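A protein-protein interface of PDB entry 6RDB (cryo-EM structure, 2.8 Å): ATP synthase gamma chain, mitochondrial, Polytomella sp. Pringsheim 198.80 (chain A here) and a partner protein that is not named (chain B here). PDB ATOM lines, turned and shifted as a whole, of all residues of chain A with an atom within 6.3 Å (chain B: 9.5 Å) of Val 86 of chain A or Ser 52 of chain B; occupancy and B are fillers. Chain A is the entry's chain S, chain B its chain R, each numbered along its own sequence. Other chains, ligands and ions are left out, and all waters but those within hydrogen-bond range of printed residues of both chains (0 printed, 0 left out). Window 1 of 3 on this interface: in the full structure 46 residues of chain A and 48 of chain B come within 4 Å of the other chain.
OG of Ser 52 of chain B sits at hydrogen-bond distance from OD1 of Asp 91 of chain A. OG1 of Thr 55 of chain B sits at hydrogen-bond distance from OD2 of Asp 83 of chain A, 3.1 Å away. The backbone carbonyl oxygen of Val 57 of chain B is in hydrogen-bond range of the guanidinium group of Arg 87 of chain A. The side-chain carboxylate (OD1) of Asp 143 of chain B lies within salt-bridge range of the guanidinium group (NH2) of Arg 87 of chain A (2.6 Å). N of Pro 51 of chain B lies close to OD1 of Asp 91 of chain A (3.5 Å).
N of Phe 50 of chain B lies within hydrogen-bond range of OD1 of Asn 53 of chain B (2.9 Å). The backbone NH of Val 57 of chain B lies within hydrogen-bond range of the side-chain hydroxyl of Thr 55 of chain B, 3.5 Å away. NZ of Lys 58 of chain B sits at hydrogen-bond distance from O of Thr 55 of chain B (2.5 Å). The backbone NH of Asp 143 of chain B sits at hydrogen-bond distance from the backbone carbonyl oxygen of Phe 135 of chain B, at 2.7 Å. The backbone carbonyl oxygen (O) of Asp 143 of chain B sits at hydrogen-bond distance from the side-chain sulfur (SG) of Cys 145 of chain B, 3.4 Å away. The side-chain carboxylate (OD2) of Asp 83 of chain A is in salt-bridge range of the guanidinium group (NH1) of Arg 87 of chain A (3.8 Å).
Among the printed residues, pairs that only touch across the chains: Asp 83 of chain A with Tyr 75 of chain B, Pro 84 of chain A with Tyr 75 of chain B, Pro 84 of chain A with Asp 143 of chain B, Pro 84 of chain A with Cys 145 of chain B, Phe 85 of chain A with Phe 135 of chain B, Val 86 of chain A with Pro 51 of chain B, Val 86 of chain A with Ser 52 of chain B, Val 86 of chain A with Thr 55 of chain B, Arg 87 of chain A with Thr 55 of chain B, Arg 87 of chain A with Ala 59 of chain B, Arg 87 of chain A with His 137 of chain B, Leu 88 of chain A with Phe 135 of chain B, Leu 88 of chain A with His 137 of chain B, Asp 91 of chain A with Gly 29 of chain B, Asp 91 of chain A with Pro 30 of chain B and Asp 91 of chain A with Phe 50 of chain B.
Printed residues of chain B within 4 Å of Asp 83 of chain A: Thr 55 and Tyr 75. Of the printed residues of chain B, Val 86 of chain A touches Pro 51 (3.8 Å), Ser 52 (3.9 Å) and Thr 55 (3.7 Å). Gly 90 of chain A touches none of the printed residues of chain B. Of the printed residues of chain A, Pro 51 of chain B touches Val 86 and Asp 91. Ser 52 of chain B touches just these residues of chain A: Val 86 and Asp 91. Printed residues of chain A within 4 Å of Thr 55 of chain B: Asp 83 (3.1 Å), Val 86 (3.7 Å) and Arg 87 (3.5 Å). Of the printed residues of chain A, Ala 59 of chain B touches Arg 87. Of the printed residues of chain A, Tyr 75 of chain B touches Asp 83 and Pro 84. The nearest residue of chain A that does not touch Ser 52 of chain B is Gly 90 of chain A (5.0 Å).
Of the 21 printed residues of chain B, 13 touch a printed residue of chain A. Of the 11 printed residues of chain A, 7 touch a printed residue of chain B. Hydrophobic or aromatic side chains of chain A that line the printed part of chain B: Pro 84, Phe 85, Val 86 and Leu 88. Among the printed residues, 21 pairs touch across the chains. Among the printed residues, Asp or Glu carboxylates within 4 Å of a Lys or Arg side-chain nitrogen of the other chain: Arg 87 of chain A with Asp 143 of chain B (2.6 Å).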
ATOM      1  N   VAL A  82       6.953  27.643 -29.490  1.00  0.00           N
ATOM      2  CA  VAL A  82       6.327  26.327 -29.564  1.00  0.00           C
ATOM      3  C   VAL A  82       4.817  26.450 -29.721  1.00  0.00           C
ATOM      4  O   VAL A  82       4.227  25.852 -30.627  1.00  0.00           O
ATOM      5  CB  VAL A  82       6.693  25.488 -28.330  1.00  0.00           C
ATOM      6  CG1 VAL A  82       6.027  24.136 -28.402  1.00  0.00           C
ATOM      7  CG2 VAL A  82       8.186  25.336 -28.239  1.00  0.00           C
ATOM      8  N   ASP A  83       4.163  27.213 -28.839  1.00  0.00           N
ATOM      9  CA  ASP A  83       2.701  27.187 -28.835  1.00  0.00           C
ATOM     10  C   ASP A  83       1.906  27.789 -30.012  1.00  0.00           C
ATOM     11  O   ASP A  83       0.735  27.408 -30.132  1.00  0.00           O
ATOM     12  CB  ASP A  83       2.137  27.712 -27.500  1.00  0.00           C
ATOM     13  CG  ASP A  83       2.509  29.139 -27.165  1.00  0.00           C
ATOM     14  OD1 ASP A  83       3.315  29.755 -27.850  1.00  0.00           O
ATOM     15  OD2 ASP A  83       1.959  29.662 -26.172  1.00  0.00           O
ATOM     16  N   PRO A  84       2.396  28.697 -30.887  1.00  0.00           N
ATOM     17  CA  PRO A  84       1.554  29.034 -32.048  1.00  0.00           C
ATOM     18  C   PRO A  84       1.415  27.902 -33.047  1.00  0.00           C
ATOM     19  O   PRO A  84       0.479  27.919 -33.853  1.00  0.00           O
ATOM     20  CB  PRO A  84       2.275  30.233 -32.668  1.00  0.00           C
ATOM     21  CG  PRO A  84       3.629  30.001 -32.356  1.00  0.00           C
ATOM     22  CD  PRO A  84       3.621  29.517 -30.962  1.00  0.00           C
ATOM     23  N   PHE A  85       2.317  26.927 -33.033  1.00  0.00           N
ATOM     24  CA  PHE A  85       2.125  25.739 -33.842  1.00  0.00           C
ATOM     25  C   PHE A  85       1.230  24.713 -33.169  1.00  0.00           C
ATOM     26  O   PHE A  85       0.662  23.862 -33.861  1.00  0.00           O
ATOM     27  CB  PHE A  85       3.461  25.081 -34.153  1.00  0.00           C
ATOM     28  CG  PHE A  85       4.394  25.937 -34.934  1.00  0.00           C
ATOM     29  CD1 PHE A  85       4.266  26.050 -36.304  1.00  0.00           C
ATOM     30  CD2 PHE A  85       5.418  26.612 -34.301  1.00  0.00           C
ATOM     31  CE1 PHE A  85       5.133  26.836 -37.022  1.00  0.00           C
ATOM     32  CE2 PHE A  85       6.288  27.399 -35.017  1.00  0.00           C
ATOM     33  CZ  PHE A  85       6.143  27.511 -36.374  1.00  0.00           C
ATOM     34  N   VAL A  86       1.099  24.751 -31.839  1.00  0.00           N
ATOM     35  CA  VAL A  86       0.247  23.773 -31.174  1.00  0.00           C
ATOM     36  C   VAL A  86      -1.198  24.244 -31.152  1.00  0.00           C
ATOM     37  O   VAL A  86      -2.098  23.449 -30.847  1.00  0.00           O
ATOM     38  CB  VAL A  86       0.743  23.451 -29.746  1.00  0.00           C
ATOM     39  CG1 VAL A  86       0.235  24.455 -28.725  1.00  0.00           C
ATOM     40  CG2 VAL A  86       0.413  22.013 -29.351  1.00  0.00           C
ATOM     41  N   ARG A  87      -1.457  25.508 -31.486  1.00  0.00           N
ATOM     42  CA  ARG A  87      -2.820  25.974 -31.663  1.00  0.00           C
ATOM     43  C   ARG A  87      -3.200  26.154 -33.123  1.00  0.00           C
ATOM     44  O   ARG A  87      -4.388  26.314 -33.418  1.00  0.00           O
ATOM     45  CB  ARG A  87      -3.054  27.290 -30.907  1.00  0.00           C
ATOM     46  CG  ARG A  87      -2.172  28.444 -31.300  1.00  0.00           C
ATOM     47  CD  ARG A  87      -2.659  29.692 -30.599  1.00  0.00           C
ATOM     48  NE  ARG A  87      -1.655  30.745 -30.527  1.00  0.00           N
ATOM     49  CZ  ARG A  87      -0.934  31.006 -29.445  1.00  0.00           C
ATOM     50  NH1 ARG A  87      -1.105  30.282 -28.351  1.00  0.00           N
ATOM     51  NH2 ARG A  87      -0.045  31.987 -29.455  1.00  0.00           N
ATOM     52  N   LEU A  88      -2.239  26.124 -34.038  1.00  0.00           N
ATOM     53  CA  LEU A  88      -2.559  26.095 -35.456  1.00  0.00           C
ATOM     54  C   LEU A  88      -2.777  24.675 -35.952  1.00  0.00           C
ATOM     55  O   LEU A  88      -3.718  24.420 -36.708  1.00  0.00           O
ATOM     56  CB  LEU A  88      -1.441  26.751 -36.266  1.00  0.00           C
ATOM     57  CG  LEU A  88      -1.762  27.110 -37.713  1.00  0.00           C
ATOM     58  CD1 LEU A  88      -2.555  28.397 -37.780  1.00  0.00           C
ATOM     59  CD2 LEU A  88      -0.490  27.221 -38.514  1.00  0.00           C
ATOM     60  N   PHE A  89      -1.919  23.748 -35.533  1.00  0.00           N
ATOM     61  CA  PHE A  89      -1.985  22.358 -35.953  1.00  0.00           C
ATOM     62  C   PHE A  89      -2.565  21.442 -34.893  1.00  0.00           C
ATOM     63  O   PHE A  89      -2.674  20.236 -35.133  1.00  0.00           O
ATOM     64  CB  PHE A  89      -0.593  21.857 -36.335  1.00  0.00           C
ATOM     65  CG  PHE A  89      -0.064  22.453 -37.592  1.00  0.00           C
ATOM     66  CD1 PHE A  89      -0.927  22.904 -38.573  1.00  0.00           C
ATOM     67  CD2 PHE A  89       1.297  22.563 -37.796  1.00  0.00           C
ATOM     68  CE1 PHE A  89      -0.442  23.456 -39.734  1.00  0.00           C
ATOM     69  CE2 PHE A  89       1.788  23.114 -38.958  1.00  0.00           C
ATOM     70  CZ  PHE A  89       0.915  23.554 -39.927  1.00  0.00           C
ATOM     71  N   GLY A  90      -2.921  21.969 -33.730  1.00  0.00           N
ATOM     72  CA  GLY A  90      -3.449  21.136 -32.677  1.00  0.00           C
ATOM     73  C   GLY A  90      -2.373  20.304 -32.001  1.00  0.00           C
ATOM     74  O   GLY A  90      -1.186  20.641 -31.982  1.00  0.00           O
ATOM     75  N   ASP A  91      -2.818  19.186 -31.436  1.00  0.00           N
ATOM     76  CA  ASP A  91      -1.946  18.235 -30.752  1.00  0.00           C
ATOM     77  C   ASP A  91      -2.559  16.859 -30.934  1.00  0.00           C
ATOM     78  O   ASP A  91      -3.580  16.551 -30.312  1.00  0.00           O
ATOM     79  CB  ASP A  91      -1.817  18.566 -29.272  1.00  0.00           C
ATOM     80  CG  ASP A  91      -0.486  18.163 -28.698  1.00  0.00           C
ATOM     81  OD1 ASP A  91      -0.001  18.884 -27.806  1.00  0.00           O
ATOM     82  OD2 ASP A  91       0.080  17.144 -29.143  1.00  0.00           O
ATOM     83  N   HIS A 250       7.722  23.519 -37.899  1.00  0.00           N
ATOM     84  CA  HIS A 250       7.173  23.026 -36.642  1.00  0.00           C
ATOM     85  C   HIS A 250       8.024  21.904 -36.070  1.00  0.00           C
ATOM     86  O   HIS A 250       8.053  21.708 -34.851  1.00  0.00           O
ATOM     87  CB  HIS A 250       5.731  22.572 -36.852  1.00  0.00           C
ATOM     88  CG  HIS A 250       5.093  21.970 -35.640  1.00  0.00           C
ATOM     89  ND1 HIS A 250       5.352  22.416 -34.364  1.00  0.00           N
ATOM     90  CD2 HIS A 250       4.150  21.009 -35.517  1.00  0.00           C
ATOM     91  CE1 HIS A 250       4.621  21.733 -33.504  1.00  0.00           C
ATOM     92  NE2 HIS A 250       3.886  20.868 -34.176  1.00  0.00           N
ATOM     93  N   GLY B  29      -5.782  13.492 -29.942  1.00  0.00           N
ATOM     94  CA  GLY B  29      -5.855  14.562 -28.981  1.00  0.00           C
ATOM     95  C   GLY B  29      -5.098  14.215 -27.722  1.00  0.00           C
ATOM     96  O   GLY B  29      -4.713  13.063 -27.504  1.00  0.00           O
ATOM     97  N   PRO B  30      -4.847  15.213 -26.871  1.00  0.00           N
ATOM     98  CA  PRO B  30      -4.174  14.913 -25.599  1.00  0.00           C
ATOM     99  C   PRO B  30      -5.064  14.169 -24.621  1.00  0.00           C
ATOM    100  O   PRO B  30      -4.568  13.337 -23.852  1.00  0.00           O
ATOM    101  CB  PRO B  30      -3.779  16.303 -25.076  1.00  0.00           C
ATOM    102  CG  PRO B  30      -4.712  17.243 -25.741  1.00  0.00           C
ATOM    103  CD  PRO B  30      -5.014  16.660 -27.086  1.00  0.00           C
ATOM    104  N   LYS B  31      -6.370  14.443 -24.637  1.00  0.00           N
ATOM    105  CA  LYS B  31      -7.281  13.792 -23.702  1.00  0.00           C
ATOM    106  C   LYS B  31      -7.500  12.328 -24.062  1.00  0.00           C
ATOM    107  O   LYS B  31      -7.513  11.464 -23.180  1.00  0.00           O
ATOM    108  CB  LYS B  31      -8.615  14.535 -23.667  1.00  0.00           C
ATOM    109  CG  LYS B  31      -9.605  13.983 -22.661  1.00  0.00           C
ATOM    110  CD  LYS B  31     -10.568  15.054 -22.193  1.00  0.00           C
ATOM    111  CE  LYS B  31     -11.718  14.450 -21.411  1.00  0.00           C
ATOM    112  NZ  LYS B  31     -11.295  14.006 -20.056  1.00  0.00           N
ATOM    113  N   PRO B  48       2.502  10.985 -20.092  1.00  0.00           N
ATOM    114  CA  PRO B  48       3.385  12.070 -20.525  1.00  0.00           C
ATOM    115  C   PRO B  48       2.611  13.350 -20.765  1.00  0.00           C
ATOM    116  O   PRO B  48       1.439  13.337 -21.143  1.00  0.00           O
ATOM    117  CB  PRO B  48       3.994  11.537 -21.828  1.00  0.00           C
ATOM    118  CG  PRO B  48       3.130  10.399 -22.229  1.00  0.00           C
ATOM    119  CD  PRO B  48       2.667   9.800 -20.950  1.00  0.00           C
ATOM    120  N   GLU B  49       3.278  14.470 -20.519  1.00  0.00           N
ATOM    121  CA  GLU B  49       2.669  15.756 -20.796  1.00  0.00           C
ATOM    122  C   GLU B  49       2.690  16.041 -22.293  1.00  0.00           C
ATOM    123  O   GLU B  49       3.332  15.343 -23.080  1.00  0.00           O
ATOM    124  CB  GLU B  49       3.383  16.863 -20.030  1.00  0.00           C
ATOM    125  CG  GLU B  49       3.257  16.745 -18.531  1.00  0.00           C
ATOM    126  CD  GLU B  49       1.854  17.010 -18.035  1.00  0.00           C
ATOM    127  OE1 GLU B  49       1.206  17.947 -18.541  1.00  0.00           O
ATOM    128  OE2 GLU B  49       1.394  16.270 -17.141  1.00  0.00           O
ATOM    129  N   PHE B  50       1.959  17.075 -22.684  1.00  0.00           N
ATOM    130  CA  PHE B  50       1.808  17.475 -24.071  1.00  0.00           C
ATOM    131  C   PHE B  50       1.967  18.983 -24.171  1.00  0.00           C
ATOM    132  O   PHE B  50       1.737  19.694 -23.189  1.00  0.00           O
ATOM    133  CB  PHE B  50       0.435  17.053 -24.614  1.00  0.00           C
ATOM    134  CG  PHE B  50       0.071  15.639 -24.291  1.00  0.00           C
ATOM    135  CD1 PHE B  50      -0.794  15.357 -23.250  1.00  0.00           C
ATOM    136  CD2 PHE B  50       0.607  14.591 -25.019  1.00  0.00           C
ATOM    137  CE1 PHE B  50      -1.128  14.056 -22.945  1.00  0.00           C
ATOM    138  CE2 PHE B  50       0.278  13.287 -24.719  1.00  0.00           C
ATOM    139  CZ  PHE B  50      -0.590  13.021 -23.677  1.00  0.00           C
ATOM    140  N   PRO B  51       2.373  19.503 -25.336  1.00  0.00           N
ATOM    141  CA  PRO B  51       2.507  20.964 -25.478  1.00  0.00           C
ATOM    142  C   PRO B  51       1.191  21.735 -25.422  1.00  0.00           C
ATOM    143  O   PRO B  51       1.235  22.969 -25.336  1.00  0.00           O
ATOM    144  CB  PRO B  51       3.193  21.130 -26.840  1.00  0.00           C
ATOM    145  CG  PRO B  51       3.109  19.801 -27.507  1.00  0.00           C
ATOM    146  CD  PRO B  51       3.041  18.784 -26.435  1.00  0.00           C
ATOM    147  N   SER B  52       0.035  21.068 -25.458  1.00  0.00           N
ATOM    148  CA  SER B  52      -1.228  21.756 -25.205  1.00  0.00           C
ATOM    149  C   SER B  52      -1.404  22.148 -23.748  1.00  0.00           C
ATOM    150  O   SER B  52      -2.136  23.099 -23.462  1.00  0.00           O
ATOM    151  CB  SER B  52      -2.408  20.889 -25.632  1.00  0.00           C
ATOM    152  OG  SER B  52      -2.459  20.774 -27.033  1.00  0.00           O
ATOM    153  N   ASN B  53      -0.760  21.442 -22.821  1.00  0.00           N
ATOM    154  CA  ASN B  53      -0.950  21.721 -21.405  1.00  0.00           C
ATOM    155  C   ASN B  53      -0.161  22.929 -20.924  1.00  0.00           C
ATOM    156  O   ASN B  53      -0.320  23.330 -19.767  1.00  0.00           O
ATOM    157  CB  ASN B  53      -0.570  20.495 -20.574  1.00  0.00           C
ATOM    158  CG  ASN B  53      -1.096  19.206 -21.169  1.00  0.00           C
ATOM    159  OD1 ASN B  53      -0.347  18.255 -21.380  1.00  0.00           O
ATOM    160  ND2 ASN B  53      -2.391  19.168 -21.445  1.00  0.00           N
ATOM    161  N   TYR B  54       0.669  23.527 -21.775  1.00  0.00           N
ATOM    162  CA  TYR B  54       1.501  24.655 -21.385  1.00  0.00           C
ATOM    163  C   TYR B  54       1.089  25.955 -22.055  1.00  0.00           C
ATOM    164  O   TYR B  54       1.862  26.918 -22.041  1.00  0.00           O
ATOM    165  CB  TYR B  54       2.964  24.348 -21.684  1.00  0.00           C
ATOM    166  CG  TYR B  54       3.431  23.100 -20.990  1.00  0.00           C
ATOM    167  CD1 TYR B  54       3.673  23.102 -19.624  1.00  0.00           C
ATOM    168  CD2 TYR B  54       3.609  21.915 -21.691  1.00  0.00           C
ATOM    169  CE1 TYR B  54       4.090  21.964 -18.977  1.00  0.00           C
ATOM    170  CE2 TYR B  54       4.027  20.767 -21.050  1.00  0.00           C
ATOM    171  CZ  TYR B  54       4.266  20.803 -19.693  1.00  0.00           C
ATOM    172  OH  TYR B  54       4.689  19.677 -19.038  1.00  0.00           O
ATOM    173  N   THR B  55      -0.097  26.008 -22.649  1.00  0.00           N
ATOM    174  CA  THR B  55      -0.610  27.240 -23.230  1.00  0.00           C
ATOM    175  C   THR B  55      -2.116  27.310 -23.030  1.00  0.00           C
ATOM    176  O   THR B  55      -2.824  26.308 -23.183  1.00  0.00           O
ATOM    177  CB  THR B  55      -0.223  27.366 -24.714  1.00  0.00           C
ATOM    178  OG1 THR B  55      -0.747  28.585 -25.256  1.00  0.00           O
ATOM    179  CG2 THR B  55      -0.677  26.170 -25.548  1.00  0.00           C
ATOM    180  N   ALA B  56      -2.587  28.478 -22.610  1.00  0.00           N
ATOM    181  CA  ALA B  56      -4.010  28.725 -22.448  1.00  0.00           C
ATOM    182  C   ALA B  56      -4.623  29.433 -23.645  1.00  0.00           C
ATOM    183  O   ALA B  56      -5.849  29.406 -23.801  1.00  0.00           O
ATOM    184  CB  ALA B  56      -4.257  29.549 -21.181  1.00  0.00           C
ATOM    185  N   VAL B  57      -3.807  30.052 -24.490  1.00  0.00           N
ATOM    186  CA  VAL B  57      -4.292  30.841 -25.615  1.00  0.00           C
ATOM    187  C   VAL B  57      -4.519  29.898 -26.787  1.00  0.00           C
ATOM    188  O   VAL B  57      -3.567  29.367 -27.363  1.00  0.00           O
ATOM    189  CB  VAL B  57      -3.306  31.955 -25.981  1.00  0.00           C
ATOM    190  CG1 VAL B  57      -3.957  32.941 -26.931  1.00  0.00           C
ATOM    191  CG2 VAL B  57      -2.813  32.653 -24.720  1.00  0.00           C
ATOM    192  N   LYS B  58      -5.776  29.688 -27.142  1.00  0.00           N
ATOM    193  CA  LYS B  58      -6.127  28.787 -28.221  1.00  0.00           C
ATOM    194  C   LYS B  58      -6.521  29.594 -29.457  1.00  0.00           C
ATOM    195  O   LYS B  58      -6.492  30.829 -29.462  1.00  0.00           O
ATOM    196  CB  LYS B  58      -7.236  27.835 -27.767  1.00  0.00           C
ATOM    197  CG  LYS B  58      -6.725  26.534 -27.159  1.00  0.00           C
ATOM    198  CD  LYS B  58      -6.312  26.719 -25.707  1.00  0.00           C
ATOM    199  CE  LYS B  58      -5.504  25.543 -25.196  1.00  0.00           C
ATOM    200  NZ  LYS B  58      -5.133  25.718 -23.765  1.00  0.00           N
ATOM    201  N   ALA B  59      -6.892  28.891 -30.525  1.00  0.00           N
ATOM    202  CA  ALA B  59      -7.265  29.519 -31.785  1.00  0.00           C
ATOM    203  C   ALA B  59      -8.755  29.809 -31.873  1.00  0.00           C
ATOM    204  O   ALA B  59      -9.151  30.939 -32.170  1.00  0.00           O
ATOM    205  CB  ALA B  59      -6.842  28.630 -32.959  1.00  0.00           C
ATOM    206  N   VAL B  60      -9.597  28.800 -31.626  1.00  0.00           N
ATOM    207  CA  VAL B  60     -11.042  28.974 -31.720  1.00  0.00           C
ATOM    208  C   VAL B  60     -11.669  29.434 -30.412  1.00  0.00           C
ATOM    209  O   VAL B  60     -12.902  29.521 -30.330  1.00  0.00           O
ATOM    210  CB  VAL B  60     -11.725  27.672 -32.183  1.00  0.00           C
ATOM    211  CG1 VAL B  60     -11.299  27.323 -33.599  1.00  0.00           C
ATOM    212  CG2 VAL B  60     -11.405  26.539 -31.227  1.00  0.00           C
ATOM    213  N   TYR B  75       7.417  36.265 -31.893  1.00  0.00           N
ATOM    214  CA  TYR B  75       8.289  35.247 -31.332  1.00  0.00           C
ATOM    215  C   TYR B  75       9.574  35.130 -32.133  1.00  0.00           C
ATOM    216  O   TYR B  75       9.731  35.737 -33.192  1.00  0.00           O
ATOM    217  CB  TYR B  75       7.618  33.889 -31.315  1.00  0.00           C
ATOM    218  CG  TYR B  75       6.535  33.730 -30.294  1.00  0.00           C
ATOM    219  CD1 TYR B  75       6.690  34.209 -29.006  1.00  0.00           C
ATOM    220  CD2 TYR B  75       5.353  33.086 -30.619  1.00  0.00           C
ATOM    221  CE1 TYR B  75       5.690  34.055 -28.068  1.00  0.00           C
ATOM    222  CE2 TYR B  75       4.346  32.931 -29.696  1.00  0.00           C
ATOM    223  CZ  TYR B  75       4.526  33.404 -28.418  1.00  0.00           C
ATOM    224  OH  TYR B  75       3.520  33.244 -27.498  1.00  0.00           O
ATOM    225  N   PHE B 135       0.774  34.122 -38.179  1.00  0.00           N
ATOM    226  CA  PHE B 135      -0.559  33.544 -38.172  1.00  0.00           C
ATOM    227  C   PHE B 135      -1.504  34.517 -37.491  1.00  0.00           C
ATOM    228  O   PHE B 135      -1.180  35.057 -36.431  1.00  0.00           O
ATOM    229  CB  PHE B 135      -0.569  32.210 -37.437  1.00  0.00           C
ATOM    230  CG  PHE B 135       0.588  31.346 -37.770  1.00  0.00           C
ATOM    231  CD1 PHE B 135       0.690  30.723 -38.995  1.00  0.00           C
ATOM    232  CD2 PHE B 135       1.590  31.158 -36.843  1.00  0.00           C
ATOM    233  CE1 PHE B 135       1.784  29.939 -39.287  1.00  0.00           C
ATOM    234  CE2 PHE B 135       2.666  30.366 -37.127  1.00  0.00           C
ATOM    235  CZ  PHE B 135       2.770  29.762 -38.345  1.00  0.00           C
ATOM    236  N   HIS B 137      -5.098  34.071 -35.933  1.00  0.00           N
ATOM    237  CA  HIS B 137      -6.018  33.018 -35.546  1.00  0.00           C
ATOM    238  C   HIS B 137      -7.439  33.568 -35.498  1.00  0.00           C
ATOM    239  O   HIS B 137      -7.627  34.787 -35.454  1.00  0.00           O
ATOM    240  CB  HIS B 137      -5.577  32.442 -34.203  1.00  0.00           C
ATOM    241  CG  HIS B 137      -4.386  31.546 -34.310  1.00  0.00           C
ATOM    242  ND1 HIS B 137      -3.106  31.966 -34.023  1.00  0.00           N
ATOM    243  CD2 HIS B 137      -4.277  30.261 -34.722  1.00  0.00           C
ATOM    244  CE1 HIS B 137      -2.263  30.971 -34.232  1.00  0.00           C
ATOM    245  NE2 HIS B 137      -2.949  29.925 -34.652  1.00  0.00           N
ATOM    246  N   ASP B 143       0.359  35.813 -34.316  1.00  0.00           N
ATOM    247  CA  ASP B 143       1.474  34.975 -33.886  1.00  0.00           C
ATOM    248  C   ASP B 143       2.579  35.068 -34.928  1.00  0.00           C
ATOM    249  O   ASP B 143       2.674  34.209 -35.804  1.00  0.00           O
ATOM    250  CB  ASP B 143       1.015  33.545 -33.705  1.00  0.00           C
ATOM    251  CG  ASP B 143       0.332  33.321 -32.387  1.00  0.00           C
ATOM    252  OD1 ASP B 143       1.000  33.456 -31.344  1.00  0.00           O
ATOM    253  OD2 ASP B 143      -0.870  33.000 -32.387  1.00  0.00           O
ATOM    254  N   CYS B 145       6.181  34.567 -36.322  1.00  0.00           N
ATOM    255  CA  CYS B 145       7.096  33.455 -36.064  1.00  0.00           C
ATOM    256  C   CYS B 145       8.267  33.544 -37.029  1.00  0.00           C
ATOM    257  O   CYS B 145       8.244  32.912 -38.085  1.00  0.00           O
ATOM    258  CB  CYS B 145       6.367  32.136 -36.226  1.00  0.00           C
ATOM    259  SG  CYS B 145       5.016  31.907 -35.091  1.00  0.00           S
